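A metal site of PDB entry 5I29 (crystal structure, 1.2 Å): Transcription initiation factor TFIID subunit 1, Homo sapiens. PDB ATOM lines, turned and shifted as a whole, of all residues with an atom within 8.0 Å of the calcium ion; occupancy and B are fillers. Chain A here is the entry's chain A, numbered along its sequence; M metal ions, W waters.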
ATOM      1  N   GLU A 134     -25.486   9.988  26.323  1.00  0.00           N
ATOM      2  CA  GLU A 134     -24.075   9.975  26.647  1.00  0.00           C
ATOM      3  C   GLU A 134     -23.275  10.147  25.351  1.00  0.00           C
ATOM      4  O   GLU A 134     -22.208  10.848  25.382  1.00  0.00           O
ATOM      5  CB  GLU A 134     -23.751   8.653  27.376  1.00  0.00           C
ATOM      6  CG  GLU A 134     -22.300   8.507  27.756  1.00  0.00           C
ATOM      7  CD  GLU A 134     -21.930   8.961  29.155  1.00  0.00           C
ATOM      8  OE1 GLU A 134     -21.136   8.261  29.812  1.00  0.00           O
ATOM      9  OE2 GLU A 134     -22.411   9.938  29.632  1.00  0.00           O
ATOM     10  N   ALA A 135     -23.584   9.442  24.317  1.00  0.00           N
ATOM     11  CA  ALA A 135     -22.847   9.549  23.078  1.00  0.00           C
ATOM     12  C   ALA A 135     -22.930  10.960  22.525  1.00  0.00           C
ATOM     13  O   ALA A 135     -21.877  11.504  22.033  1.00  0.00           O
ATOM     14  CB  ALA A 135     -23.470   8.574  22.097  1.00  0.00           C
ATOM     15  N   GLU A 136     -24.061  11.619  22.615  1.00  0.00           N
ATOM     16  CA  GLU A 136     -24.233  13.021  22.120  1.00  0.00           C
ATOM     17  C   GLU A 136     -23.353  13.928  22.886  1.00  0.00           C
ATOM     18  O   GLU A 136     -22.634  14.773  22.289  1.00  0.00           O
ATOM     19  CB  GLU A 136     -25.690  13.429  22.256  1.00  0.00           C
ATOM     20  CG  GLU A 136     -26.676  12.675  21.379  1.00  0.00           C
ATOM     21  CD  GLU A 136     -28.139  12.875  21.696  1.00  0.00           C
ATOM     22  OE1 GLU A 136     -28.428  13.208  22.882  1.00  0.00           O
ATOM     23  OE2 GLU A 136     -29.001  12.686  20.829  1.00  0.00           O
ATOM     24  N   LEU A 137     -23.279  13.772  24.214  1.00  0.00           N
ATOM     25  CA  LEU A 137     -22.470  14.626  25.063  1.00  0.00           C
ATOM     26  C   LEU A 137     -20.999  14.358  24.843  1.00  0.00           C
ATOM     27  O   LEU A 137     -20.196  15.319  24.826  1.00  0.00           O
ATOM     28  CB  LEU A 137     -22.788  14.386  26.546  1.00  0.00           C
ATOM     29  CG  LEU A 137     -24.225  14.898  26.951  1.00  0.00           C
ATOM     30  CD1 LEU A 137     -24.691  14.298  28.287  1.00  0.00           C
ATOM     31  CD2 LEU A 137     -24.301  16.401  27.025  1.00  0.00           C
ATOM     32  N   GLU A 138     -20.595  13.119  24.681  1.00  0.00           N
ATOM     33  CA  GLU A 138     -19.192  12.798  24.470  1.00  0.00           C
ATOM     34  C   GLU A 138     -18.709  13.375  23.119  1.00  0.00           C
ATOM     35  O   GLU A 138     -17.524  13.833  22.993  1.00  0.00           O
ATOM     36  CB  GLU A 138     -18.952  11.285  24.399  1.00  0.00           C
ATOM     37  CG  GLU A 138     -18.956  10.537  25.767  1.00  0.00           C
ATOM     38  CD  GLU A 138     -17.826  10.896  26.677  1.00  0.00           C
ATOM     39  OE1 GLU A 138     -16.945  11.681  26.310  1.00  0.00           O
ATOM     40  OE2 GLU A 138     -17.842  10.394  27.859  1.00  0.00           O
ATOM     41  N   SER A 139     -19.541  13.398  22.088  1.00  0.00           N
ATOM     42  CA  SER A 139     -19.114  13.994  20.791  1.00  0.00           C
ATOM     43  C   SER A 139     -19.058  15.484  20.911  1.00  0.00           C
ATOM     44  O   SER A 139     -18.100  16.105  20.403  1.00  0.00           O
ATOM     45  CB  SER A 139     -20.162  13.554  19.811  1.00  0.00           C
ATOM     46  OG  SER A 139     -19.788  14.167  18.530  1.00  0.00           O
ATOM     47  N   LEU A 140     -20.055  16.127  21.570  1.00  0.00           N
ATOM     48  CA  LEU A 140     -20.166  17.543  21.578  1.00  0.00           C
ATOM     49  C   LEU A 140     -19.060  18.163  22.228  1.00  0.00           C
ATOM     50  O   LEU A 140     -18.647  19.298  21.737  1.00  0.00           O
ATOM     51  CB  LEU A 140     -21.513  17.986  22.179  1.00  0.00           C
ATOM     52  CG  LEU A 140     -21.885  19.427  22.057  1.00  0.00           C
ATOM     53  CD1 LEU A 140     -21.980  19.765  20.558  1.00  0.00           C
ATOM     54  CD2 LEU A 140     -23.257  19.587  22.713  1.00  0.00           C
ATOM     55  N   ASP A 141     -18.450  17.554  23.217  1.00  0.00           N
ATOM     56  CA  ASP A 141     -17.214  18.174  23.650  1.00  0.00           C
ATOM     57  C   ASP A 141     -16.146  17.546  22.800  1.00  0.00           C
ATOM     58  O   ASP A 141     -15.880  16.344  22.906  1.00  0.00           O
ATOM     59  CB  ASP A 141     -17.094  17.761  25.050  1.00  0.00           C
ATOM     60  CG  ASP A 141     -15.853  18.287  25.680  1.00  0.00           C
ATOM     61  OD1 ASP A 141     -14.955  18.774  24.950  1.00  0.00           O
ATOM     62  OD2 ASP A 141     -15.775  18.279  26.920  1.00  0.00           O
ATOM     63  N   PRO A 142     -15.455  18.339  21.979  1.00  0.00           N
ATOM     64  CA  PRO A 142     -14.417  17.744  21.038  1.00  0.00           C
ATOM     65  C   PRO A 142     -13.149  17.291  21.774  1.00  0.00           C
ATOM     66  O   PRO A 142     -12.283  16.659  21.120  1.00  0.00           O
ATOM     67  CB  PRO A 142     -14.186  18.882  19.996  1.00  0.00           C
ATOM     68  CG  PRO A 142     -14.294  20.086  20.927  1.00  0.00           C
ATOM     69  CD  PRO A 142     -15.503  19.823  21.792  1.00  0.00           C
ATOM     70  N   MET A 143     -12.981  17.598  23.066  1.00  0.00           N
ATOM     71  CA  MET A 143     -11.901  17.020  23.931  1.00  0.00           C
ATOM     72  C   MET A 143     -12.114  15.534  24.255  1.00  0.00           C
ATOM     73  O   MET A 143     -13.248  14.967  24.241  1.00  0.00           O
ATOM     74  CB  MET A 143     -11.756  17.784  25.192  1.00  0.00           C
ATOM     75  CG  MET A 143     -11.521  19.255  24.963  1.00  0.00           C
ATOM     76  SD  MET A 143      -9.943  19.646  24.206  1.00  0.00           S
ATOM     77  CE  MET A 143      -9.729  21.321  24.848  1.00  0.00           C
ATOM     78  N   THR A 144     -11.013  14.865  24.613  1.00  0.00           N
ATOM     79  CA  THR A 144     -11.047  13.499  25.106  1.00  0.00           C
ATOM     80  C   THR A 144      -9.641  12.990  25.475  1.00  0.00           C
ATOM     81  O   THR A 144      -8.959  13.625  26.274  1.00  0.00           O
ATOM     82  CB  THR A 144     -11.625  12.558  24.069  1.00  0.00           C
ATOM     83  OG1 THR A 144     -12.094  11.373  24.741  1.00  0.00           O
ATOM     84  CG2 THR A 144     -10.565  12.228  23.011  1.00  0.00           C
HETATM   85 CA    CA M   1     -15.365  14.270  23.613  1.00  0.00          CA
HETATM   86  O   HOH W   1     -15.939  14.450  25.876  1.00  0.00           O
HETATM   87  O   HOH W   2     -14.643  13.778  21.454  1.00  0.00           O
HETATM   88  O   HOH W   3     -15.118  12.044  24.131  1.00  0.00           O
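Water W3 lies within hydrogen-bond range of the side-chain carboxylate (OE1) of Glu 138 (2.9 Å) and the side-chain hydroxyl (OG1) of Thr 144 (3.2 Å).
The calcium ion is bound by O of Asp 141 (2.3 Å), O of Glu 138 (2.3 Å), water W3 (2.3 Å), O of Met 143 (2.3 Å), water W2 (2.3 Å) and water W1 (2.3 Å).
Within 4 Å of the calcium ion: Glu 138, Asp 141 and Met 143.
Along chain A the residues within 4 Å of the calcium ion span positions 138 to 143.
The side-chain carboxylate of Asp 141 lies within hydrogen-bond range of the backbone NH of Met 143.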
